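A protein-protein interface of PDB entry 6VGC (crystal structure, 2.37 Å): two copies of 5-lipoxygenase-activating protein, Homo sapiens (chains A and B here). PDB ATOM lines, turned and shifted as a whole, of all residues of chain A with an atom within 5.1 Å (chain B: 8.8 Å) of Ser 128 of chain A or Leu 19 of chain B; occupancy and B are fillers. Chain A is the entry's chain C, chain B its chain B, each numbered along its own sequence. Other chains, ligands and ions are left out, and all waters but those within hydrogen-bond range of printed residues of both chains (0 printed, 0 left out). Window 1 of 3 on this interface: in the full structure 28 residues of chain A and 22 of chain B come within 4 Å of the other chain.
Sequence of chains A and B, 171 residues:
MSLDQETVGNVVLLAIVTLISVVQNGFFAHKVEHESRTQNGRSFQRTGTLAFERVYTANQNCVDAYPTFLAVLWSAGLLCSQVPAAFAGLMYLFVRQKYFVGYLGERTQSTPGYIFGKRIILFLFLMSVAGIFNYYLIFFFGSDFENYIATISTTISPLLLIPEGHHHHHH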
ATOM      1  N   VAL A  72     -12.333 -16.362 -16.104  1.00  0.00           N
ATOM      2  CA  VAL A  72     -10.976 -16.060 -15.614  1.00  0.00           C
ATOM      3  C   VAL A  72     -10.550 -16.950 -14.448  1.00  0.00           C
ATOM      4  O   VAL A  72      -9.367 -17.254 -14.311  1.00  0.00           O
ATOM      5  CB  VAL A  72     -10.735 -14.554 -15.273  1.00  0.00           C
ATOM      6  CG1 VAL A  72     -10.608 -13.733 -16.537  1.00  0.00           C
ATOM      7  CG2 VAL A  72     -11.814 -13.990 -14.356  1.00  0.00           C
ATOM      8  N   SER A  75      -9.608 -20.271 -16.266  1.00  0.00           N
ATOM      9  CA  SER A  75      -8.399 -20.002 -17.046  1.00  0.00           C
ATOM     10  C   SER A  75      -7.171 -19.955 -16.132  1.00  0.00           C
ATOM     11  O   SER A  75      -6.196 -20.670 -16.358  1.00  0.00           O
ATOM     12  CB  SER A  75      -8.525 -18.695 -17.832  1.00  0.00           C
ATOM     13  OG  SER A  75      -9.499 -18.805 -18.850  1.00  0.00           O
ATOM     14  N   ALA A  76      -7.237 -19.130 -15.089  1.00  0.00           N
ATOM     15  CA  ALA A  76      -6.132 -19.001 -14.135  1.00  0.00           C
ATOM     16  C   ALA A  76      -5.813 -20.320 -13.425  1.00  0.00           C
ATOM     17  O   ALA A  76      -4.654 -20.714 -13.334  1.00  0.00           O
ATOM     18  CB  ALA A  76      -6.426 -17.906 -13.126  1.00  0.00           C
ATOM     19  N   LEU A  79      -4.459 -23.062 -16.264  1.00  0.00           N
ATOM     20  CA  LEU A  79      -3.279 -22.710 -17.059  1.00  0.00           C
ATOM     21  C   LEU A  79      -2.077 -22.266 -16.225  1.00  0.00           C
ATOM     22  O   LEU A  79      -0.935 -22.403 -16.666  1.00  0.00           O
ATOM     23  CB  LEU A  79      -3.622 -21.632 -18.096  1.00  0.00           C
ATOM     24  CG  LEU A  79      -4.777 -21.881 -19.076  1.00  0.00           C
ATOM     25  CD1 LEU A  79      -5.109 -20.604 -19.830  1.00  0.00           C
ATOM     26  CD2 LEU A  79      -4.471 -23.018 -20.047  1.00  0.00           C
ATOM     27  N   CYS A  80      -2.333 -21.738 -15.030  1.00  0.00           N
ATOM     28  CA  CYS A  80      -1.271 -21.184 -14.190  1.00  0.00           C
ATOM     29  C   CYS A  80      -1.039 -22.010 -12.923  1.00  0.00           C
ATOM     30  O   CYS A  80      -0.127 -22.838 -12.881  1.00  0.00           O
ATOM     31  CB  CYS A  80      -1.570 -19.720 -13.851  1.00  0.00           C
ATOM     32  SG  CYS A  80      -0.210 -18.815 -13.078  1.00  0.00           S
ATOM     33  N   LEU A 124      -6.615 -12.436 -11.770  1.00  0.00           N
ATOM     34  CA  LEU A 124      -6.949 -13.718 -12.391  1.00  0.00           C
ATOM     35  C   LEU A 124      -6.689 -13.704 -13.899  1.00  0.00           C
ATOM     36  O   LEU A 124      -6.233 -14.701 -14.462  1.00  0.00           O
ATOM     37  CB  LEU A 124      -8.402 -14.107 -12.090  1.00  0.00           C
ATOM     38  CG  LEU A 124      -8.706 -14.516 -10.645  1.00  0.00           C
ATOM     39  CD1 LEU A 124     -10.191 -14.406 -10.342  1.00  0.00           C
ATOM     40  CD2 LEU A 124      -8.190 -15.917 -10.338  1.00  0.00           C
ATOM     41  N   PHE A 125      -6.971 -12.571 -14.539  1.00  0.00           N
ATOM     42  CA  PHE A 125      -6.655 -12.371 -15.956  1.00  0.00           C
ATOM     43  C   PHE A 125      -5.142 -12.428 -16.190  1.00  0.00           C
ATOM     44  O   PHE A 125      -4.685 -13.004 -17.179  1.00  0.00           O
ATOM     45  CB  PHE A 125      -7.227 -11.035 -16.452  1.00  0.00           C
ATOM     46  CG  PHE A 125      -6.876 -10.707 -17.880  1.00  0.00           C
ATOM     47  CD1 PHE A 125      -5.749  -9.941 -18.177  1.00  0.00           C
ATOM     48  CD2 PHE A 125      -7.675 -11.152 -18.927  1.00  0.00           C
ATOM     49  CE1 PHE A 125      -5.418  -9.634 -19.496  1.00  0.00           C
ATOM     50  CE2 PHE A 125      -7.355 -10.852 -20.248  1.00  0.00           C
ATOM     51  CZ  PHE A 125      -6.223 -10.091 -20.533  1.00  0.00           C
ATOM     52  N   LEU A 126      -4.382 -11.827 -15.274  1.00  0.00           N
ATOM     53  CA  LEU A 126      -2.921 -11.806 -15.344  1.00  0.00           C
ATOM     54  C   LEU A 126      -2.315 -13.196 -15.180  1.00  0.00           C
ATOM     55  O   LEU A 126      -1.360 -13.545 -15.874  1.00  0.00           O
ATOM     56  CB  LEU A 126      -2.342 -10.834 -14.306  1.00  0.00           C
ATOM     57  CG  LEU A 126      -1.926  -9.422 -14.754  1.00  0.00           C
ATOM     58  CD1 LEU A 126      -2.960  -8.733 -15.646  1.00  0.00           C
ATOM     59  CD2 LEU A 126      -1.600  -8.551 -13.545  1.00  0.00           C
ATOM     60  N   MET A 127      -2.879 -13.983 -14.264  1.00  0.00           N
ATOM     61  CA  MET A 127      -2.494 -15.382 -14.084  1.00  0.00           C
ATOM     62  C   MET A 127      -2.715 -16.205 -15.351  1.00  0.00           C
ATOM     63  O   MET A 127      -1.914 -17.083 -15.674  1.00  0.00           O
ATOM     64  CB  MET A 127      -3.285 -16.013 -12.939  1.00  0.00           C
ATOM     65  CG  MET A 127      -2.832 -15.618 -11.549  1.00  0.00           C
ATOM     66  SD  MET A 127      -3.766 -16.502 -10.287  1.00  0.00           S
ATOM     67  CE  MET A 127      -3.025 -18.133 -10.367  1.00  0.00           C
ATOM     68  N   SER A 128      -3.803 -15.917 -16.062  1.00  0.00           N
ATOM     69  CA  SER A 128      -4.146 -16.637 -17.289  1.00  0.00           C
ATOM     70  C   SER A 128      -3.161 -16.334 -18.418  1.00  0.00           C
ATOM     71  O   SER A 128      -2.799 -17.224 -19.191  1.00  0.00           O
ATOM     72  CB  SER A 128      -5.574 -16.307 -17.729  1.00  0.00           C
ATOM     73  OG  SER A 128      -6.496 -16.506 -16.672  1.00  0.00           O
ATOM     74  N   VAL A 129      -2.732 -15.077 -18.501  1.00  0.00           N
ATOM     75  CA  VAL A 129      -1.733 -14.648 -19.482  1.00  0.00           C
ATOM     76  C   VAL A 129      -0.368 -15.258 -19.144  1.00  0.00           C
ATOM     77  O   VAL A 129       0.322 -15.774 -20.023  1.00  0.00           O
ATOM     78  CB  VAL A 129      -1.658 -13.098 -19.584  1.00  0.00           C
ATOM     79  CG1 VAL A 129      -0.580 -12.661 -20.567  1.00  0.00           C
ATOM     80  CG2 VAL A 129      -3.005 -12.530 -20.010  1.00  0.00           C
ATOM     81  N   ALA A 130      -0.004 -15.212 -17.863  1.00  0.00           N
ATOM     82  CA  ALA A 130       1.227 -15.830 -17.367  1.00  0.00           C
ATOM     83  C   ALA A 130       1.251 -17.335 -17.629  1.00  0.00           C
ATOM     84  O   ALA A 130       2.305 -17.902 -17.921  1.00  0.00           O
ATOM     85  CB  ALA A 130       1.396 -15.552 -15.881  1.00  0.00           C
ATOM     86  N   GLY A 131       0.083 -17.968 -17.519  1.00  0.00           N
ATOM     87  CA  GLY A 131      -0.071 -19.393 -17.792  1.00  0.00           C
ATOM     88  C   GLY A 131       0.109 -19.748 -19.256  1.00  0.00           C
ATOM     89  O   GLY A 131       0.738 -20.759 -19.582  1.00  0.00           O
ATOM     90  N   ILE A 132      -0.445 -18.918 -20.139  1.00  0.00           N
ATOM     91  CA  ILE A 132      -0.315 -19.111 -21.586  1.00  0.00           C
ATOM     92  C   ILE A 132       1.134 -18.917 -22.043  1.00  0.00           C
ATOM     93  O   ILE A 132       1.643 -19.705 -22.845  1.00  0.00           O
ATOM     94  CB  ILE A 132      -1.287 -18.200 -22.374  1.00  0.00           C
ATOM     95  CG1 ILE A 132      -2.725 -18.699 -22.196  1.00  0.00           C
ATOM     96  CG2 ILE A 132      -0.927 -18.157 -23.860  1.00  0.00           C
ATOM     97  CD1 ILE A 132      -3.782 -17.660 -22.478  1.00  0.00           C
ATOM     98  N   VAL B   8      -3.342 -28.433 -22.976  1.00  0.00           N
ATOM     99  CA  VAL B   8      -3.274 -26.978 -23.148  1.00  0.00           C
ATOM    100  C   VAL B   8      -3.148 -26.616 -24.630  1.00  0.00           C
ATOM    101  O   VAL B   8      -3.785 -25.674 -25.098  1.00  0.00           O
ATOM    102  CB  VAL B   8      -2.123 -26.335 -22.324  1.00  0.00           C
ATOM    103  CG1 VAL B   8      -2.126 -24.818 -22.484  1.00  0.00           C
ATOM    104  CG2 VAL B   8      -2.245 -26.700 -20.852  1.00  0.00           C
ATOM    105  N   VAL B  11      -6.353 -26.411 -26.352  1.00  0.00           N
ATOM    106  CA  VAL B  11      -7.286 -25.403 -25.826  1.00  0.00           C
ATOM    107  C   VAL B  11      -6.737 -23.969 -25.780  1.00  0.00           C
ATOM    108  O   VAL B  11      -7.469 -23.035 -25.437  1.00  0.00           O
ATOM    109  CB  VAL B  11      -7.832 -25.789 -24.413  1.00  0.00           C
ATOM    110  CG1 VAL B  11      -8.515 -27.150 -24.440  1.00  0.00           C
ATOM    111  CG2 VAL B  11      -6.729 -25.765 -23.364  1.00  0.00           C
ATOM    112  N   VAL B  12      -5.464 -23.796 -26.136  1.00  0.00           N
ATOM    113  CA  VAL B  12      -4.782 -22.502 -25.967  1.00  0.00           C
ATOM    114  C   VAL B  12      -5.423 -21.376 -26.786  1.00  0.00           C
ATOM    115  O   VAL B  12      -5.560 -20.256 -26.300  1.00  0.00           O
ATOM    116  CB  VAL B  12      -3.238 -22.605 -26.216  1.00  0.00           C
ATOM    117  CG1 VAL B  12      -2.912 -22.894 -27.687  1.00  0.00           C
ATOM    118  CG2 VAL B  12      -2.511 -21.350 -25.721  1.00  0.00           C
ATOM    119  N   LEU B  13      -5.837 -21.689 -28.011  1.00  0.00           N
ATOM    120  CA  LEU B  13      -6.457 -20.708 -28.898  1.00  0.00           C
ATOM    121  C   LEU B  13      -7.842 -20.306 -28.399  1.00  0.00           C
ATOM    122  O   LEU B  13      -8.203 -19.126 -28.431  1.00  0.00           O
ATOM    123  CB  LEU B  13      -6.531 -21.243 -30.335  1.00  0.00           C
ATOM    124  CG  LEU B  13      -5.247 -21.755 -31.004  1.00  0.00           C
ATOM    125  CD1 LEU B  13      -5.563 -22.372 -32.357  1.00  0.00           C
ATOM    126  CD2 LEU B  13      -4.196 -20.656 -31.150  1.00  0.00           C
ATOM    127  N   LEU B  14      -8.610 -21.291 -27.935  1.00  0.00           N
ATOM    128  CA  LEU B  14      -9.928 -21.039 -27.361  1.00  0.00           C
ATOM    129  C   LEU B  14      -9.797 -20.207 -26.084  1.00  0.00           C
ATOM    130  O   LEU B  14     -10.598 -19.303 -25.840  1.00  0.00           O
ATOM    131  CB  LEU B  14     -10.672 -22.353 -27.083  1.00  0.00           C
ATOM    132  CG  LEU B  14     -10.902 -23.335 -28.240  1.00  0.00           C
ATOM    133  CD1 LEU B  14     -11.363 -24.683 -27.704  1.00  0.00           C
ATOM    134  CD2 LEU B  14     -11.890 -22.799 -29.278  1.00  0.00           C
ATOM    135  N   ALA B  15      -8.778 -20.514 -25.282  1.00  0.00           N
ATOM    136  CA  ALA B  15      -8.456 -19.725 -24.087  1.00  0.00           C
ATOM    137  C   ALA B  15      -8.139 -18.266 -24.431  1.00  0.00           C
ATOM    138  O   ALA B  15      -8.625 -17.350 -23.767  1.00  0.00           O
ATOM    139  CB  ALA B  15      -7.298 -20.360 -23.317  1.00  0.00           C
ATOM    140  N   ILE B  16      -7.336 -18.060 -25.476  1.00  0.00           N
ATOM    141  CA  ILE B  16      -6.970 -16.710 -25.930  1.00  0.00           C
ATOM    142  C   ILE B  16      -8.196 -15.906 -26.386  1.00  0.00           C
ATOM    143  O   ILE B  16      -8.401 -14.781 -25.929  1.00  0.00           O
ATOM    144  CB  ILE B  16      -5.861 -16.742 -27.029  1.00  0.00           C
ATOM    145  CG1 ILE B  16      -4.532 -17.217 -26.425  1.00  0.00           C
ATOM    146  CG2 ILE B  16      -5.684 -15.361 -27.669  1.00  0.00           C
ATOM    147  CD1 ILE B  16      -3.520 -17.746 -27.441  1.00  0.00           C
ATOM    148  N   VAL B  17      -9.007 -16.497 -27.266  1.00  0.00           N
ATOM    149  CA  VAL B  17     -10.271 -15.899 -27.712  1.00  0.00           C
ATOM    150  C   VAL B  17     -11.189 -15.577 -26.523  1.00  0.00           C
ATOM    151  O   VAL B  17     -11.857 -14.540 -26.512  1.00  0.00           O
ATOM    152  CB  VAL B  17     -11.010 -16.809 -28.747  1.00  0.00           C
ATOM    153  CG1 VAL B  17     -12.422 -16.302 -29.030  1.00  0.00           C
ATOM    154  CG2 VAL B  17     -10.221 -16.900 -30.046  1.00  0.00           C
ATOM    155  N   THR B  18     -11.205 -16.463 -25.528  1.00  0.00           N
ATOM    156  CA  THR B  18     -12.003 -16.273 -24.312  1.00  0.00           C
ATOM    157  C   THR B  18     -11.498 -15.091 -23.475  1.00  0.00           C
ATOM    158  O   THR B  18     -12.291 -14.296 -22.964  1.00  0.00           O
ATOM    159  CB  THR B  18     -12.051 -17.570 -23.454  1.00  0.00           C
ATOM    160  OG1 THR B  18     -12.620 -18.632 -24.227  1.00  0.00           O
ATOM    161  CG2 THR B  18     -12.892 -17.378 -22.199  1.00  0.00           C
ATOM    162  N   LEU B  19     -10.180 -14.975 -23.345  1.00  0.00           N
ATOM    163  CA  LEU B  19      -9.578 -13.883 -22.572  1.00  0.00           C
ATOM    164  C   LEU B  19      -9.711 -12.512 -23.240  1.00  0.00           C
ATOM    165  O   LEU B  19      -9.728 -11.488 -22.555  1.00  0.00           O
ATOM    166  CB  LEU B  19      -8.115 -14.187 -22.252  1.00  0.00           C
ATOM    167  CG  LEU B  19      -7.880 -15.241 -21.166  1.00  0.00           C
ATOM    168  CD1 LEU B  19      -6.439 -15.688 -21.184  1.00  0.00           C
ATOM    169  CD2 LEU B  19      -8.266 -14.719 -19.784  1.00  0.00           C
ATOM    170  N   ILE B  20      -9.802 -12.497 -24.570  1.00  0.00           N
ATOM    171  CA  ILE B  20     -10.044 -11.260 -25.312  1.00  0.00           C
ATOM    172  C   ILE B  20     -11.503 -10.824 -25.131  1.00  0.00           C
ATOM    173  O   ILE B  20     -11.789  -9.628 -25.023  1.00  0.00           O
ATOM    174  CB  ILE B  20      -9.675 -11.387 -26.822  1.00  0.00           C
ATOM    175  CG1 ILE B  20      -8.202 -11.780 -26.993  1.00  0.00           C
ATOM    176  CG2 ILE B  20      -9.940 -10.075 -27.561  1.00  0.00           C
ATOM    177  CD1 ILE B  20      -7.833 -12.251 -28.393  1.00  0.00           C
ATOM    178  N   SER B  21     -12.413 -11.800 -25.086  1.00  0.00           N
ATOM    179  CA  SER B  21     -13.826 -11.538 -24.803  1.00  0.00           C
ATOM    180  C   SER B  21     -14.017 -11.007 -23.384  1.00  0.00           C
ATOM    181  O   SER B  21     -14.909 -10.196 -23.135  1.00  0.00           O
ATOM    182  CB  SER B  21     -14.685 -12.790 -25.038  1.00  0.00           C
ATOM    183  OG  SER B  21     -14.443 -13.799 -24.070  1.00  0.00           O
ATOM    184  N   VAL B  22     -13.176 -11.471 -22.462  1.00  0.00           N
ATOM    185  CA  VAL B  22     -13.143 -10.951 -21.093  1.00  0.00           C
ATOM    186  C   VAL B  22     -12.764  -9.464 -21.103  1.00  0.00           C
ATOM    187  O   VAL B  22     -13.452  -8.646 -20.488  1.00  0.00           O
ATOM    188  CB  VAL B  22     -12.190 -11.783 -20.185  1.00  0.00           C
ATOM    189  CG1 VAL B  22     -11.869 -11.045 -18.886  1.00  0.00           C
ATOM    190  CG2 VAL B  22     -12.799 -13.146 -19.884  1.00  0.00           C
ATOM    191  N   VAL B  23     -11.688  -9.126 -21.820  1.00  0.00           N
ATOM    192  CA  VAL B  23     -11.266  -7.731 -22.012  1.00  0.00           C
ATOM    193  C   VAL B  23     -12.403  -6.891 -22.603  1.00  0.00           C
ATOM    194  O   VAL B  23     -12.671  -5.782 -22.135  1.00  0.00           O
ATOM    195  CB  VAL B  23      -9.998  -7.623 -22.912  1.00  0.00           C
ATOM    196  CG1 VAL B  23      -9.698  -6.165 -23.281  1.00  0.00           C
ATOM    197  CG2 VAL B  23      -8.795  -8.238 -22.224  1.00  0.00           C
ATOM    198  N   GLN B  24     -13.072  -7.438 -23.618  1.00  0.00           N
ATOM    199  CA  GLN B  24     -14.203  -6.772 -24.263  1.00  0.00           C
ATOM    200  C   GLN B  24     -15.391  -6.575 -23.309  1.00  0.00           C
ATOM    201  O   GLN B  24     -16.024  -5.520 -23.324  1.00  0.00           O
ATOM    202  CB  GLN B  24     -14.633  -7.535 -25.525  1.00  0.00           C
ATOM    203  CG  GLN B  24     -15.525  -6.731 -26.465  1.00  0.00           C
ATOM    204  CD  GLN B  24     -15.963  -7.511 -27.694  1.00  0.00           C
ATOM    205  OE1 GLN B  24     -16.098  -8.734 -27.658  1.00  0.00           O
ATOM    206  NE2 GLN B  24     -16.196  -6.800 -28.790  1.00  0.00           N
ATOM    207  N   ASN B  25     -15.687  -7.588 -22.491  1.00  0.00           N
ATOM    208  CA  ASN B  25     -16.728  -7.477 -21.464  1.00  0.00           C
ATOM    209  C   ASN B  25     -16.408  -6.367 -20.466  1.00  0.00           C
ATOM    210  O   ASN B  25     -17.283  -5.568 -20.116  1.00  0.00           O
ATOM    211  CB  ASN B  25     -16.924  -8.805 -20.721  1.00  0.00           C
ATOM    212  CG  ASN B  25     -17.551  -9.886 -21.595  1.00  0.00           C
ATOM    213  OD1 ASN B  25     -18.185  -9.600 -22.611  1.00  0.00           O
ATOM    214  ND2 ASN B  25     -17.369 -11.139 -21.196  1.00  0.00           N
ATOM    215  N   GLY B  26     -15.151  -6.330 -20.023  1.00  0.00           N
ATOM    216  CA  GLY B  26     -14.651  -5.279 -19.142  1.00  0.00           C
ATOM    217  C   GLY B  26     -14.758  -3.898 -19.761  1.00  0.00           C
ATOM    218  O   GLY B  26     -15.134  -2.943 -19.083  1.00  0.00           O
ATOM    219  N   TYR B  66     -23.674 -13.720 -24.131  1.00  0.00           N
ATOM    220  CA  TYR B  66     -22.331 -14.224 -23.832  1.00  0.00           C
ATOM    221  C   TYR B  66     -22.231 -15.686 -23.375  1.00  0.00           C
ATOM    222  O   TYR B  66     -21.370 -16.418 -23.870  1.00  0.00           O
ATOM    223  CB  TYR B  66     -21.609 -13.287 -22.850  1.00  0.00           C
ATOM    224  CG  TYR B  66     -20.147 -13.623 -22.631  1.00  0.00           C
ATOM    225  CD1 TYR B  66     -19.224 -13.530 -23.677  1.00  0.00           C
ATOM    226  CD2 TYR B  66     -19.684 -14.016 -21.379  1.00  0.00           C
ATOM    227  CE1 TYR B  66     -17.883 -13.830 -23.480  1.00  0.00           C
ATOM    228  CE2 TYR B  66     -18.341 -14.317 -21.172  1.00  0.00           C
ATOM    229  CZ  TYR B  66     -17.449 -14.223 -22.226  1.00  0.00           C
ATOM    230  OH  TYR B  66     -16.122 -14.521 -22.030  1.00  0.00           O
ATOM    231  N   PHE B  69     -22.550 -17.848 -26.255  1.00  0.00           N
ATOM    232  CA  PHE B  69     -21.319 -17.752 -27.042  1.00  0.00           C
ATOM    233  C   PHE B  69     -20.214 -18.676 -26.529  1.00  0.00           C
ATOM    234  O   PHE B  69     -19.625 -19.421 -27.310  1.00  0.00           O
ATOM    235  CB  PHE B  69     -20.814 -16.302 -27.122  1.00  0.00           C
ATOM    236  CG  PHE B  69     -19.433 -16.174 -27.713  1.00  0.00           C
ATOM    237  CD1 PHE B  69     -19.178 -16.581 -29.023  1.00  0.00           C
ATOM    238  CD2 PHE B  69     -18.389 -15.658 -26.960  1.00  0.00           C
ATOM    239  CE1 PHE B  69     -17.902 -16.476 -29.567  1.00  0.00           C
ATOM    240  CE2 PHE B  69     -17.107 -15.546 -27.495  1.00  0.00           C
ATOM    241  CZ  PHE B  69     -16.863 -15.953 -28.801  1.00  0.00           C
ATOM    242  N   LEU B  70     -19.930 -18.623 -25.226  1.00  0.00           N
ATOM    243  CA  LEU B  70     -18.912 -19.484 -24.622  1.00  0.00           C
ATOM    244  C   LEU B  70     -19.251 -20.963 -24.772  1.00  0.00           C
ATOM    245  O   LEU B  70     -18.389 -21.772 -25.122  1.00  0.00           O
ATOM    246  CB  LEU B  70     -18.688 -19.142 -23.142  1.00  0.00           C
ATOM    247  CG  LEU B  70     -17.959 -17.848 -22.759  1.00  0.00           C
ATOM    248  CD1 LEU B  70     -17.632 -17.869 -21.269  1.00  0.00           C
ATOM    249  CD2 LEU B  70     -16.684 -17.622 -23.579  1.00  0.00           C
ATOM    250  N   LEU B  73     -18.656 -21.909 -28.419  1.00  0.00           N
ATOM    251  CA  LEU B  73     -17.249 -21.732 -28.765  1.00  0.00           C
ATOM    252  C   LEU B  73     -16.441 -22.941 -28.303  1.00  0.00           C
ATOM    253  O   LEU B  73     -15.696 -23.534 -29.090  1.00  0.00           O
ATOM    254  CB  LEU B  73     -16.697 -20.433 -28.154  1.00  0.00           C
ATOM    255  CG  LEU B  73     -15.192 -20.122 -28.188  1.00  0.00           C
ATOM    256  CD1 LEU B  73     -14.687 -19.827 -29.601  1.00  0.00           C
ATOM    257  CD2 LEU B  73     -14.874 -18.958 -27.266  1.00  0.00           C
ATOM    258  N   TRP B  74     -16.609 -23.309 -27.034  1.00  0.00           N
ATOM    259  CA  TRP B  74     -15.865 -24.421 -26.450  1.00  0.00           C
ATOM    260  C   TRP B  74     -16.334 -25.782 -26.969  1.00  0.00           C
ATOM    261  O   TRP B  74     -15.508 -26.648 -27.265  1.00  0.00           O
ATOM    262  CB  TRP B  74     -15.858 -24.333 -24.916  1.00  0.00           C
ATOM    263  CG  TRP B  74     -14.928 -23.245 -24.412  1.00  0.00           C
ATOM    264  CD1 TRP B  74     -15.235 -21.928 -24.221  1.00  0.00           C
ATOM    265  CD2 TRP B  74     -13.542 -23.387 -24.072  1.00  0.00           C
ATOM    266  NE1 TRP B  74     -14.128 -21.241 -23.769  1.00  0.00           N
ATOM    267  CE2 TRP B  74     -13.076 -22.113 -23.669  1.00  0.00           C
ATOM    268  CE3 TRP B  74     -12.649 -24.468 -24.059  1.00  0.00           C
ATOM    269  CZ2 TRP B  74     -11.756 -21.890 -23.260  1.00  0.00           C
ATOM    270  CZ3 TRP B  74     -11.334 -24.246 -23.653  1.00  0.00           C
ATOM    271  CH2 TRP B  74     -10.902 -22.964 -23.259  1.00  0.00           C
ATOM    272  N   LEU B  90     -13.334 -15.324 -32.723  1.00  0.00           N
ATOM    273  CA  LEU B  90     -12.679 -14.025 -32.887  1.00  0.00           C
ATOM    274  C   LEU B  90     -13.493 -13.090 -33.785  1.00  0.00           C
ATOM    275  O   LEU B  90     -13.500 -11.873 -33.582  1.00  0.00           O
ATOM    276  CB  LEU B  90     -11.262 -14.203 -33.439  1.00  0.00           C
ATOM    277  CG  LEU B  90     -10.246 -13.093 -33.148  1.00  0.00           C
ATOM    278  CD1 LEU B  90      -9.792 -13.118 -31.692  1.00  0.00           C
ATOM    279  CD2 LEU B  90      -9.049 -13.216 -34.078  1.00  0.00           C
ATOM    280  N   LEU B  93     -16.271 -11.509 -31.737  1.00  0.00           N
ATOM    281  CA  LEU B  93     -15.791 -10.369 -30.951  1.00  0.00           C
ATOM    282  C   LEU B  93     -15.719  -9.094 -31.791  1.00  0.00           C
ATOM    283  O   LEU B  93     -15.927  -7.993 -31.278  1.00  0.00           O
ATOM    284  CB  LEU B  93     -14.434 -10.673 -30.302  1.00  0.00           C
ATOM    285  CG  LEU B  93     -14.350 -11.915 -29.402  1.00  0.00           C
ATOM    286  CD1 LEU B  93     -12.961 -12.086 -28.808  1.00  0.00           C
ATOM    287  CD2 LEU B  93     -15.393 -11.874 -28.303  1.00  0.00           C
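No position is printed for both chains.
Of the 14 printed residues of chain A, 5 touch a printed residue of chain B. Of the 24 printed residues of chain B, 4 touch a printed residue of chain A. Hydrophobic or aromatic side chains of chain B within 4 Å of the printed part of chain A: Val 8, Leu 19, Val 22 and Val 23. Among the printed residues, 6 pairs touch across the chains. Among the printed residues, no Asp or Glu carboxylate lies within 4 Å of a Lys or Arg side-chain nitrogen of the other chain.
O of Leu 124 of chain A is in hydrogen-bond range of OG of Ser 128 of chain A. The backbone NH (N) of Ala 76 of chain A sits at hydrogen-bond distance from the side-chain hydroxyl (OG) of Ser 128 of chain A, at 3.2 Å.
Among the printed residues, pairs that only touch across the chains: Phe 125 of chain A with Leu 19 of chain B, Ile 132 of chain A with Leu 19 of chain B, Phe 125 of chain A with Val 23 of chain B, Ser 128 of chain A with Leu 19 of chain B, Val 72 of chain A with Val 22 of chain B and Leu 79 of chain A with Val 8 of chain B.
Of the printed residues of chain B, Val 72 of chain A touches Val 22 (3.8 Å). Of the printed residues of chain B, Leu 79 of chain A touches Val 8. Of the printed residues of chain B, Phe 125 of chain A touches Leu 19 and Val 23. Ser 128 of chain A touches one residue of chain B. Of the printed residues of chain A, Val 8 of chain B touches Leu 79. Of the printed residues of chain A, Leu 19 of chain B touches Phe 125, Ser 128 and Ile 132. Printed residues of chain A within 4 Å of Val 23 of chain B: Phe 125. Leu 70 of chain B touches none of the printed residues of chain A.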
